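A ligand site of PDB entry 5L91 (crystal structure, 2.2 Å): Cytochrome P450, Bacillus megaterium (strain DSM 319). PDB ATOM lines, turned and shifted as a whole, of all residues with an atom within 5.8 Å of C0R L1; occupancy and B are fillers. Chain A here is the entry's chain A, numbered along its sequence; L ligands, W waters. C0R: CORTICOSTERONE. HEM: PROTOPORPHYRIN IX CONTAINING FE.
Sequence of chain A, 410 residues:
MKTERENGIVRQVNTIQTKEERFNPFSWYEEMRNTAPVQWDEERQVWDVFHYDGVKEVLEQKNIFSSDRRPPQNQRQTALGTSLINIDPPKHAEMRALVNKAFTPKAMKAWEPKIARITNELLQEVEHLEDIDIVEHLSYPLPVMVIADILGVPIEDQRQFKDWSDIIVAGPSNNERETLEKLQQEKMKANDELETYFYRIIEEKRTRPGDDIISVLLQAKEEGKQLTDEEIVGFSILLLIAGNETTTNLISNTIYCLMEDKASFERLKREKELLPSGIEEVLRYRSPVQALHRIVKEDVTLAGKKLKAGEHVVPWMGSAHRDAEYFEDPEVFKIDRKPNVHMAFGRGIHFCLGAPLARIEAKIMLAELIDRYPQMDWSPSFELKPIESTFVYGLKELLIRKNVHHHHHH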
ATOM      1  N   ILE A  85      -5.845  -9.077 -23.307  1.00  0.00           N
ATOM      2  CA  ILE A  85      -4.655  -8.852 -22.506  1.00  0.00           C
ATOM      3  C   ILE A  85      -3.381  -9.079 -23.279  1.00  0.00           C
ATOM      4  O   ILE A  85      -2.292  -8.701 -22.797  1.00  0.00           O
ATOM      5  CB  ILE A  85      -4.740  -9.753 -21.260  1.00  0.00           C
ATOM      6  CG1 ILE A  85      -3.805  -9.242 -20.194  1.00  0.00           C
ATOM      7  CG2 ILE A  85      -4.366 -11.240 -21.601  1.00  0.00           C
ATOM      8  CD1 ILE A  85      -4.054  -9.856 -18.808  1.00  0.00           C
ATOM      9  N   ILE A 168      -7.775 -25.838 -15.938  1.00  0.00           N
ATOM     10  CA  ILE A 168      -7.017 -24.749 -16.523  1.00  0.00           C
ATOM     11  C   ILE A 168      -6.022 -24.164 -15.536  1.00  0.00           C
ATOM     12  O   ILE A 168      -5.010 -23.593 -15.940  1.00  0.00           O
ATOM     13  CB  ILE A 168      -8.011 -23.751 -17.133  1.00  0.00           C
ATOM     14  CG1 ILE A 168      -8.327 -24.266 -18.530  1.00  0.00           C
ATOM     15  CG2 ILE A 168      -7.448 -22.350 -17.140  1.00  0.00           C
ATOM     16  CD1 ILE A 168      -9.301 -23.464 -19.338  1.00  0.00           C
ATOM     17  N   VAL A 169      -6.260 -24.291 -14.233  1.00  0.00           N
ATOM     18  CA  VAL A 169      -5.313 -23.719 -13.267  1.00  0.00           C
ATOM     19  C   VAL A 169      -4.607 -24.786 -12.456  1.00  0.00           C
ATOM     20  O   VAL A 169      -3.932 -24.458 -11.480  1.00  0.00           O
ATOM     21  CB  VAL A 169      -5.999 -22.690 -12.349  1.00  0.00           C
ATOM     22  CG1 VAL A 169      -6.722 -21.655 -13.164  1.00  0.00           C
ATOM     23  CG2 VAL A 169      -6.940 -23.378 -11.353  1.00  0.00           C
ATOM     24  N   ALA A 170      -4.710 -26.049 -12.852  1.00  0.00           N
ATOM     25  CA  ALA A 170      -4.115 -27.121 -12.055  1.00  0.00           C
ATOM     26  C   ALA A 170      -2.588 -27.084 -12.130  1.00  0.00           C
ATOM     27  O   ALA A 170      -2.008 -26.643 -13.122  1.00  0.00           O
ATOM     28  CB  ALA A 170      -4.640 -28.492 -12.508  1.00  0.00           C
ATOM     29  N   LYS A 187      -5.053 -29.347 -20.263  1.00  0.00           N
ATOM     30  CA  LYS A 187      -5.367 -27.921 -20.356  1.00  0.00           C
ATOM     31  C   LYS A 187      -5.794 -27.543 -21.763  1.00  0.00           C
ATOM     32  O   LYS A 187      -6.741 -26.774 -21.942  1.00  0.00           O
ATOM     33  CB  LYS A 187      -4.168 -27.076 -19.925  1.00  0.00           C
ATOM     34  CG  LYS A 187      -3.794 -27.289 -18.468  1.00  0.00           C
ATOM     35  CD  LYS A 187      -2.978 -26.123 -17.880  1.00  0.00           C
ATOM     36  CE  LYS A 187      -2.602 -26.405 -16.434  1.00  0.00           C
ATOM     37  NZ  LYS A 187      -2.256 -25.152 -15.728  1.00  0.00           N
ATOM     38  N   ILE A 241      -9.641 -16.957 -16.455  1.00  0.00           N
ATOM     39  CA  ILE A 241      -8.268 -17.136 -16.094  1.00  0.00           C
ATOM     40  C   ILE A 241      -7.777 -15.931 -15.303  1.00  0.00           C
ATOM     41  O   ILE A 241      -7.035 -16.081 -14.358  1.00  0.00           O
ATOM     42  CB  ILE A 241      -7.425 -17.376 -17.342  1.00  0.00           C
ATOM     43  CG1 ILE A 241      -7.733 -18.787 -17.889  1.00  0.00           C
ATOM     44  CG2 ILE A 241      -5.947 -17.229 -17.017  1.00  0.00           C
ATOM     45  CD1 ILE A 241      -7.401 -18.921 -19.262  1.00  0.00           C
ATOM     46  N   ALA A 242      -8.181 -14.739 -15.730  1.00  0.00           N
ATOM     47  CA  ALA A 242      -7.699 -13.507 -15.135  1.00  0.00           C
ATOM     48  C   ALA A 242      -8.382 -13.207 -13.827  1.00  0.00           C
ATOM     49  O   ALA A 242      -7.763 -12.595 -12.952  1.00  0.00           O
ATOM     50  CB  ALA A 242      -7.910 -12.370 -16.124  1.00  0.00           C
ATOM     51  N   GLU A 245      -8.461 -17.049  -9.877  1.00  0.00           N
ATOM     52  CA  GLU A 245      -7.460 -17.270  -8.848  1.00  0.00           C
ATOM     53  C   GLU A 245      -7.020 -15.955  -8.198  1.00  0.00           C
ATOM     54  O   GLU A 245      -6.703 -15.946  -7.011  1.00  0.00           O
ATOM     55  CB  GLU A 245      -6.274 -18.009  -9.418  1.00  0.00           C
ATOM     56  CG  GLU A 245      -5.301 -18.359  -8.314  1.00  0.00           C
ATOM     57  CD  GLU A 245      -4.220 -19.332  -8.736  1.00  0.00           C
ATOM     58  OE1 GLU A 245      -4.445 -20.557  -8.751  1.00  0.00           O
ATOM     59  OE2 GLU A 245      -3.139 -18.835  -9.064  1.00  0.00           O
ATOM     60  N   THR A 246      -7.018 -14.857  -8.949  1.00  0.00           N
ATOM     61  CA  THR A 246      -6.670 -13.556  -8.388  1.00  0.00           C
ATOM     62  C   THR A 246      -7.641 -13.158  -7.276  1.00  0.00           C
ATOM     63  O   THR A 246      -7.231 -12.759  -6.200  1.00  0.00           O
ATOM     64  CB  THR A 246      -6.694 -12.524  -9.492  1.00  0.00           C
ATOM     65  OG1 THR A 246      -7.894 -12.686 -10.222  1.00  0.00           O
ATOM     66  CG2 THR A 246      -5.546 -12.678 -10.407  1.00  0.00           C
ATOM     67  N   VAL A 289      -1.337 -10.553  -7.751  1.00  0.00           N
ATOM     68  CA  VAL A 289      -0.426 -10.525  -8.884  1.00  0.00           C
ATOM     69  C   VAL A 289       0.790  -9.692  -8.474  1.00  0.00           C
ATOM     70  O   VAL A 289       0.692  -8.465  -8.306  1.00  0.00           O
ATOM     71  CB  VAL A 289      -1.081  -9.963 -10.150  1.00  0.00           C
ATOM     72  CG1 VAL A 289      -0.128 -10.093 -11.354  1.00  0.00           C
ATOM     73  CG2 VAL A 289      -2.422 -10.689 -10.462  1.00  0.00           C
ATOM     74  N   ALA A 291       3.741  -9.535 -10.341  1.00  0.00           N
ATOM     75  CA  ALA A 291       4.557  -9.103 -11.452  1.00  0.00           C
ATOM     76  C   ALA A 291       3.805  -9.353 -12.756  1.00  0.00           C
ATOM     77  O   ALA A 291       2.935 -10.228 -12.842  1.00  0.00           O
ATOM     78  CB  ALA A 291       5.898  -9.839 -11.474  1.00  0.00           C
ATOM     79  N   LEU A 292       4.178  -8.609 -13.781  1.00  0.00           N
ATOM     80  CA  LEU A 292       3.625  -8.780 -15.126  1.00  0.00           C
ATOM     81  C   LEU A 292       4.728  -8.987 -16.141  1.00  0.00           C
ATOM     82  O   LEU A 292       5.884  -9.194 -15.768  1.00  0.00           O
ATOM     83  CB  LEU A 292       2.773  -7.580 -15.521  1.00  0.00           C
ATOM     84  CG  LEU A 292       1.476  -7.439 -14.731  1.00  0.00           C
ATOM     85  CD1 LEU A 292       0.826  -6.149 -15.085  1.00  0.00           C
ATOM     86  CD2 LEU A 292       0.561  -8.587 -15.032  1.00  0.00           C
ATOM     87  N   SER A 389       4.769 -20.043  -6.872  1.00  0.00           N
ATOM     88  CA  SER A 389       4.743 -19.156  -8.020  1.00  0.00           C
ATOM     89  C   SER A 389       5.496 -17.889  -7.661  1.00  0.00           C
ATOM     90  O   SER A 389       5.534 -17.512  -6.488  1.00  0.00           O
ATOM     91  CB  SER A 389       3.306 -18.802  -8.422  1.00  0.00           C
ATOM     92  OG  SER A 389       3.276 -17.782  -9.378  1.00  0.00           O
ATOM     93  N   PHE A 391       4.946 -15.127  -9.900  1.00  0.00           N
ATOM     94  CA  PHE A 391       4.062 -14.092 -10.406  1.00  0.00           C
ATOM     95  C   PHE A 391       2.797 -13.943  -9.568  1.00  0.00           C
ATOM     96  O   PHE A 391       2.161 -12.883  -9.579  1.00  0.00           O
ATOM     97  CB  PHE A 391       3.715 -14.378 -11.841  1.00  0.00           C
ATOM     98  CG  PHE A 391       4.821 -14.074 -12.771  1.00  0.00           C
ATOM     99  CD1 PHE A 391       5.883 -14.943 -12.957  1.00  0.00           C
ATOM    100  CD2 PHE A 391       4.797 -12.903 -13.459  1.00  0.00           C
ATOM    101  CE1 PHE A 391       6.902 -14.603 -13.826  1.00  0.00           C
ATOM    102  CE2 PHE A 391       5.804 -12.555 -14.318  1.00  0.00           C
ATOM    103  CZ  PHE A 391       6.861 -13.386 -14.502  1.00  0.00           C
ATOM    104  N   VAL A 392       2.406 -15.020  -8.885  1.00  0.00           N
ATOM    105  CA  VAL A 392       1.163 -15.129  -8.151  1.00  0.00           C
ATOM    106  C   VAL A 392       1.468 -15.321  -6.685  1.00  0.00           C
ATOM    107  O   VAL A 392       2.314 -16.137  -6.317  1.00  0.00           O
ATOM    108  CB  VAL A 392       0.343 -16.277  -8.761  1.00  0.00           C
ATOM    109  CG1 VAL A 392      -0.823 -16.627  -7.969  1.00  0.00           C
ATOM    110  CG2 VAL A 392      -0.093 -15.823 -10.131  1.00  0.00           C
HETATM  111  C1  C0R L   1      -3.465 -19.148 -14.400  1.00  0.00           C
HETATM  112  C2  C0R L   1      -3.512 -20.666 -14.387  1.00  0.00           C
HETATM  113  C3  C0R L   1      -2.074 -21.370 -14.509  1.00  0.00           C
HETATM  114  C4  C0R L   1      -0.779 -20.569 -13.917  1.00  0.00           C
HETATM  115  C5  C0R L   1      -1.016 -19.121 -13.465  1.00  0.00           C
HETATM  116  C6  C0R L   1       0.251 -18.312 -12.908  1.00  0.00           C
HETATM  117  C7  C0R L   1       0.281 -16.908 -13.745  1.00  0.00           C
HETATM  118  C8  C0R L   1      -1.049 -16.155 -13.600  1.00  0.00           C
HETATM  119  C9  C0R L   1      -2.312 -16.998 -14.131  1.00  0.00           C
HETATM  120  C10 C0R L   1      -2.437 -18.452 -13.566  1.00  0.00           C
HETATM  121  C11 C0R L   1      -3.659 -16.129 -14.063  1.00  0.00           C
HETATM  122  C12 C0R L   1      -3.433 -14.702 -14.803  1.00  0.00           C
HETATM  123  C13 C0R L   1      -2.251 -13.882 -14.270  1.00  0.00           C
HETATM  124  C14 C0R L   1      -0.878 -14.781 -14.273  1.00  0.00           C
HETATM  125  C15 C0R L   1       0.053 -13.965 -13.731  1.00  0.00           C
HETATM  126  C16 C0R L   1      -0.261 -12.537 -14.421  1.00  0.00           C
HETATM  127  C17 C0R L   1      -1.837 -12.799 -15.016  1.00  0.00           C
HETATM  128  C18 C0R L   1      -2.598 -13.469 -12.804  1.00  0.00           C
HETATM  129  C19 C0R L   1      -3.023 -18.527 -12.101  1.00  0.00           C
HETATM  130  C20 C0R L   1      -2.702 -11.536 -14.862  1.00  0.00           C
HETATM  131  C21 C0R L   1      -4.067 -11.451 -15.549  1.00  0.00           C
HETATM  132  O1  C0R L   1      -1.886 -22.468 -15.018  1.00  0.00           O
HETATM  133  O2  C0R L   1      -4.064 -15.947 -12.813  1.00  0.00           O
HETATM  134  O3  C0R L   1      -2.304 -10.606 -14.169  1.00  0.00           O
HETATM  135  O4  C0R L   1      -4.651 -10.251 -15.095  1.00  0.00           O
HETATM  136  C1  C0R L   2      -3.395 -16.292 -20.583  1.00  0.00           C
HETATM  137  C2  C0R L   2      -4.428 -15.568 -19.756  1.00  0.00           C
HETATM  138  C3  C0R L   2      -3.779 -14.524 -18.717  1.00  0.00           C
HETATM  139  C4  C0R L   2      -2.463 -13.710 -19.220  1.00  0.00           C
HETATM  140  C5  C0R L   2      -1.878 -14.236 -20.558  1.00  0.00           C
HETATM  141  C6  C0R L   2      -0.623 -13.480 -21.135  1.00  0.00           C
HETATM  142  C7  C0R L   2       0.315 -14.607 -21.815  1.00  0.00           C
HETATM  143  C8  C0R L   2      -0.264 -15.597 -22.776  1.00  0.00           C
HETATM  144  C9  C0R L   2      -1.417 -16.392 -22.045  1.00  0.00           C
HETATM  145  C10 C0R L   2      -2.482 -15.454 -21.369  1.00  0.00           C
HETATM  146  C11 C0R L   2      -1.972 -17.591 -22.977  1.00  0.00           C
HETATM  147  C12 C0R L   2      -0.775 -18.456 -23.669  1.00  0.00           C
HETATM  148  C13 C0R L   2       0.278 -17.610 -24.371  1.00  0.00           C
HETATM  149  C14 C0R L   2       0.870 -16.495 -23.310  1.00  0.00           C
HETATM  150  C15 C0R L   2       1.860 -15.901 -23.968  1.00  0.00           C
HETATM  151  C16 C0R L   2       2.606 -17.163 -24.635  1.00  0.00           C
HETATM  152  C17 C0R L   2       1.355 -18.332 -24.734  1.00  0.00           C
HETATM  153  C18 C0R L   2      -0.347 -16.872 -25.608  1.00  0.00           C
HETATM  154  C19 C0R L   2      -3.370 -14.847 -22.479  1.00  0.00           C
HETATM  155  C20 C0R L   2       1.213 -19.028 -26.113  1.00  0.00           C
HETATM  156  C21 C0R L   2       0.371 -20.322 -26.231  1.00  0.00           C
HETATM  157  O1  C0R L   2      -4.271 -14.296 -17.618  1.00  0.00           O
HETATM  158  O2  C0R L   2      -2.718 -17.163 -23.979  1.00  0.00           O
HETATM  159  O3  C0R L   2       1.765 -18.533 -27.084  1.00  0.00           O
HETATM  160  O4  C0R L   2       0.976 -21.359 -25.463  1.00  0.00           O
HETATM  161  CHA HEM L   3      -6.077  -7.080 -16.294  1.00  0.00           C
HETATM  162  CHB HEM L   3      -5.059  -8.091 -11.695  1.00  0.00           C
HETATM  163  CHC HEM L   3      -9.504  -9.785 -10.941  1.00  0.00           C
HETATM  164  CHD HEM L   3     -10.215  -9.443 -15.691  1.00  0.00           C
HETATM  165  C1A HEM L   3      -5.435  -7.172 -15.084  1.00  0.00           C
HETATM  166  C2A HEM L   3      -4.109  -6.692 -14.813  1.00  0.00           C
HETATM  167  C3A HEM L   3      -3.827  -6.992 -13.532  1.00  0.00           C
HETATM  168  C4A HEM L   3      -4.974  -7.660 -12.983  1.00  0.00           C
HETATM  169  CMA HEM L   3      -2.531  -6.737 -12.751  1.00  0.00           C
HETATM  170  CAA HEM L   3      -3.191  -6.010 -15.847  1.00  0.00           C
HETATM  171  CBA HEM L   3      -2.486  -7.102 -16.654  1.00  0.00           C
HETATM  172  CGA HEM L   3      -1.584  -6.443 -17.686  1.00  0.00           C
HETATM  173  O1A HEM L   3      -1.435  -5.212 -17.691  1.00  0.00           O
HETATM  174  O2A HEM L   3      -1.040  -7.140 -18.577  1.00  0.00           O
HETATM  175  C1B HEM L   3      -6.186  -8.566 -11.102  1.00  0.00           C
HETATM  176  C2B HEM L   3      -6.307  -8.804  -9.688  1.00  0.00           C
HETATM  177  C3B HEM L   3      -7.521  -9.307  -9.481  1.00  0.00           C
HETATM  178  C4B HEM L   3      -8.210  -9.341 -10.749  1.00  0.00           C
HETATM  179  CMB HEM L   3      -5.173  -8.554  -8.674  1.00  0.00           C
HETATM  180  CAB HEM L   3      -8.191  -9.734  -8.151  1.00  0.00           C
HETATM  181  CBB HEM L   3      -8.051  -9.079  -7.017  1.00  0.00           C
HETATM  182  C1C HEM L   3     -10.138  -9.809 -12.154  1.00  0.00           C
HETATM  183  C2C HEM L   3     -11.499 -10.139 -12.425  1.00  0.00           C
HETATM  184  C3C HEM L   3     -11.686 -10.015 -13.755  1.00  0.00           C
HETATM  185  C4C HEM L   3     -10.440  -9.635 -14.342  1.00  0.00           C
HETATM  186  CMC HEM L   3     -12.516 -10.490 -11.327  1.00  0.00           C
HETATM  187  CAC HEM L   3     -12.956 -10.273 -14.589  1.00  0.00           C
HETATM  188  CBC HEM L   3     -13.872 -11.143 -14.158  1.00  0.00           C
HETATM  189  C1D HEM L   3      -9.158  -8.802 -16.247  1.00  0.00           C
HETATM  190  C2D HEM L   3      -9.034  -8.531 -17.654  1.00  0.00           C
HETATM  191  C3D HEM L   3      -7.876  -7.870 -17.834  1.00  0.00           C
HETATM  192  C4D HEM L   3      -7.262  -7.726 -16.538  1.00  0.00           C
HETATM  193  CMD HEM L   3     -10.061  -8.941 -18.741  1.00  0.00           C
HETATM  194  CAD HEM L   3      -7.257  -7.369 -19.178  1.00  0.00           C
HETATM  195  CBD HEM L   3      -7.569  -5.924 -19.478  1.00  0.00           C
HETATM  196  CGD HEM L   3      -6.868  -5.443 -20.704  1.00  0.00           C
HETATM  197  O1D HEM L   3      -7.376  -4.444 -21.235  1.00  0.00           O
HETATM  198  O2D HEM L   3      -5.865  -6.064 -21.176  1.00  0.00           O
HETATM  199  NA  HEM L   3      -5.940  -7.752 -13.933  1.00  0.00           N
HETATM  200  NB  HEM L   3      -7.355  -8.910 -11.738  1.00  0.00           N
HETATM  201  NC  HEM L   3      -9.520  -9.517 -13.346  1.00  0.00           N
HETATM  202  ND  HEM L   3      -8.070  -8.282 -15.566  1.00  0.00           N
HETATM  203 FE   HEM L   3      -7.784  -8.497 -13.620  1.00  0.00          FE
HETATM  204  C1  C0R L   4       0.098 -20.705 -19.007  1.00  0.00           C
HETATM  205  C2  C0R L   4       0.618 -19.784 -17.891  1.00  0.00           C
HETATM  206  C3  C0R L   4      -0.289 -18.479 -17.778  1.00  0.00           C
HETATM  207  C4  C0R L   4      -1.879 -18.815 -17.715  1.00  0.00           C
HETATM  208  C5  C0R L   4      -2.323 -20.189 -18.303  1.00  0.00           C
HETATM  209  C6  C0R L   4      -3.876 -20.567 -18.261  1.00  0.00           C
HETATM  210  C7  C0R L   4      -4.339 -21.060 -19.745  1.00  0.00           C
HETATM  211  C8  C0R L   4      -3.348 -21.945 -20.485  1.00  0.00           C
HETATM  212  C9  C0R L   4      -1.824 -21.474 -20.409  1.00  0.00           C
HETATM  213  C10 C0R L   4      -1.300 -21.183 -18.962  1.00  0.00           C
HETATM  214  C11 C0R L   4      -0.893 -22.369 -21.367  1.00  0.00           C
HETATM  215  C12 C0R L   4      -1.476 -22.388 -22.897  1.00  0.00           C
HETATM  216  C13 C0R L   4      -2.928 -22.815 -22.986  1.00  0.00           C
HETATM  217  C14 C0R L   4      -3.893 -21.976 -21.929  1.00  0.00           C
HETATM  218  C15 C0R L   4      -5.101 -22.501 -22.108  1.00  0.00           C
HETATM  219  C16 C0R L   4      -5.196 -22.472 -23.704  1.00  0.00           C
HETATM  220  C17 C0R L   4      -3.543 -22.510 -24.164  1.00  0.00           C
HETATM  221  C18 C0R L   4      -3.004 -24.343 -22.654  1.00  0.00           C
HETATM  222  C19 C0R L   4      -1.214 -22.513 -18.137  1.00  0.00           C
HETATM  223  C20 C0R L   4      -3.345 -23.490 -25.322  1.00  0.00           C
HETATM  224  C21 C0R L   4      -2.140 -23.313 -26.298  1.00  0.00           C
HETATM  225  O1  C0R L   4       0.119 -17.321 -17.728  1.00  0.00           O
HETATM  226  O2  C0R L   4      -0.787 -23.618 -20.931  1.00  0.00           O
HETATM  227  O3  C0R L   4      -4.166 -24.389 -25.409  1.00  0.00           O
HETATM  228  O4  C0R L   4      -1.752 -24.533 -26.920  1.00  0.00           O
HETATM  229  C1  C0R L   5       3.621 -13.775 -16.652  1.00  0.00           C
HETATM  230  C2  C0R L   5       2.566 -12.702 -16.383  1.00  0.00           C
HETATM  231  C3  C0R L   5       2.117 -11.826 -17.647  1.00  0.00           C
HETATM  232  C4  C0R L   5       2.082 -12.621 -19.077  1.00  0.00           C
HETATM  233  C5  C0R L   5       2.900 -13.939 -19.131  1.00  0.00           C
HETATM  234  C6  C0R L   5       3.006 -14.810 -20.453  1.00  0.00           C
HETATM  235  C7  C0R L   5       4.530 -14.751 -20.969  1.00  0.00           C
HETATM  236  C8  C0R L   5       5.461 -15.208 -19.865  1.00  0.00           C
HETATM  237  C9  C0R L   5       5.198 -14.582 -18.432  1.00  0.00           C
HETATM  238  C10 C0R L   5       3.712 -14.499 -17.944  1.00  0.00           C
HETATM  239  C11 C0R L   5       6.195 -15.282 -17.397  1.00  0.00           C
HETATM  240  C12 C0R L   5       7.749 -15.270 -17.929  1.00  0.00           C
HETATM  241  C13 C0R L   5       7.983 -15.626 -19.403  1.00  0.00           C
HETATM  242  C14 C0R L   5       6.878 -14.918 -20.368  1.00  0.00           C
HETATM  243  C15 C0R L   5       7.152 -15.350 -21.590  1.00  0.00           C
HETATM  244  C16 C0R L   5       8.763 -15.280 -21.616  1.00  0.00           C
HETATM  245  C17 C0R L   5       9.125 -15.141 -19.963  1.00  0.00           C
HETATM  246  C18 C0R L   5       7.854 -17.184 -19.529  1.00  0.00           C
HETATM  247  C19 C0R L   5       3.132 -15.935 -17.770  1.00  0.00           C
HETATM  248  C20 C0R L   5      10.432 -15.851 -19.563  1.00  0.00           C
HETATM  249  C21 C0R L   5      11.071 -15.491 -18.206  1.00  0.00           C
HETATM  250  O1  C0R L   5       1.797 -10.640 -17.596  1.00  0.00           O
HETATM  251  O2  C0R L   5       5.784 -16.523 -17.192  1.00  0.00           O
HETATM  252  O3  C0R L   5      10.937 -16.666 -20.325  1.00  0.00           O
HETATM  253  O4  C0R L   5      11.858 -16.566 -17.737  1.00  0.00           O
HETATM  254  O   HOH W   1      -3.536 -15.833  -9.820  1.00  0.00           O
HETATM  255  O   HOH W   2      -6.935 -10.334 -13.908  1.00  0.00           O
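An oxygen (O2) of C0R L1 is in hydrogen-bond range of the backbone carbonyl oxygen (O) of Ile 241, at 3.4 Å.
The side-chain amino group (NZ) of Lys 187 is in hydrogen-bond range of an oxygen (O1) of C0R L1 (2.8 Å).
OG1 of Thr 246 lies within hydrogen-bond range of O of Ala 242, at 2.7 Å.
O of Ala 170 lies within hydrogen-bond range of NZ of Lys 187, 3.0 Å away.
OG of Ser 389 sits at hydrogen-bond distance from N of Val 392 (2.9 Å).
NZ of Lys 187 lies within hydrogen-bond range of O of Ile 168, 3.2 Å away.
An oxygen (O1) of C0R L1 lies close to the backbone carbonyl oxygen (O) of Ile 168.
Merely in contact with C0R L1: Glu 245, Val 169, Val 289, Leu 292, Val 392, Ile 85, Thr 246 and Ala 242.
Of the 15 residues printed, 11 come within 4 Å of C0R L1.
The nearest printed residue that does not touch C0R L1 is Phe 391 (4.1 Å).
Water W2 bridges an oxygen (O4) of C0R L1 (2.6 Å) and the backbone carbonyl oxygen of Ala 242 (2.6 Å).
Water W1 bridges an oxygen (O2) of C0R L1 (3.0 Å) and the side-chain carboxylate (OE2) of Glu 245 (3.1 Å).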
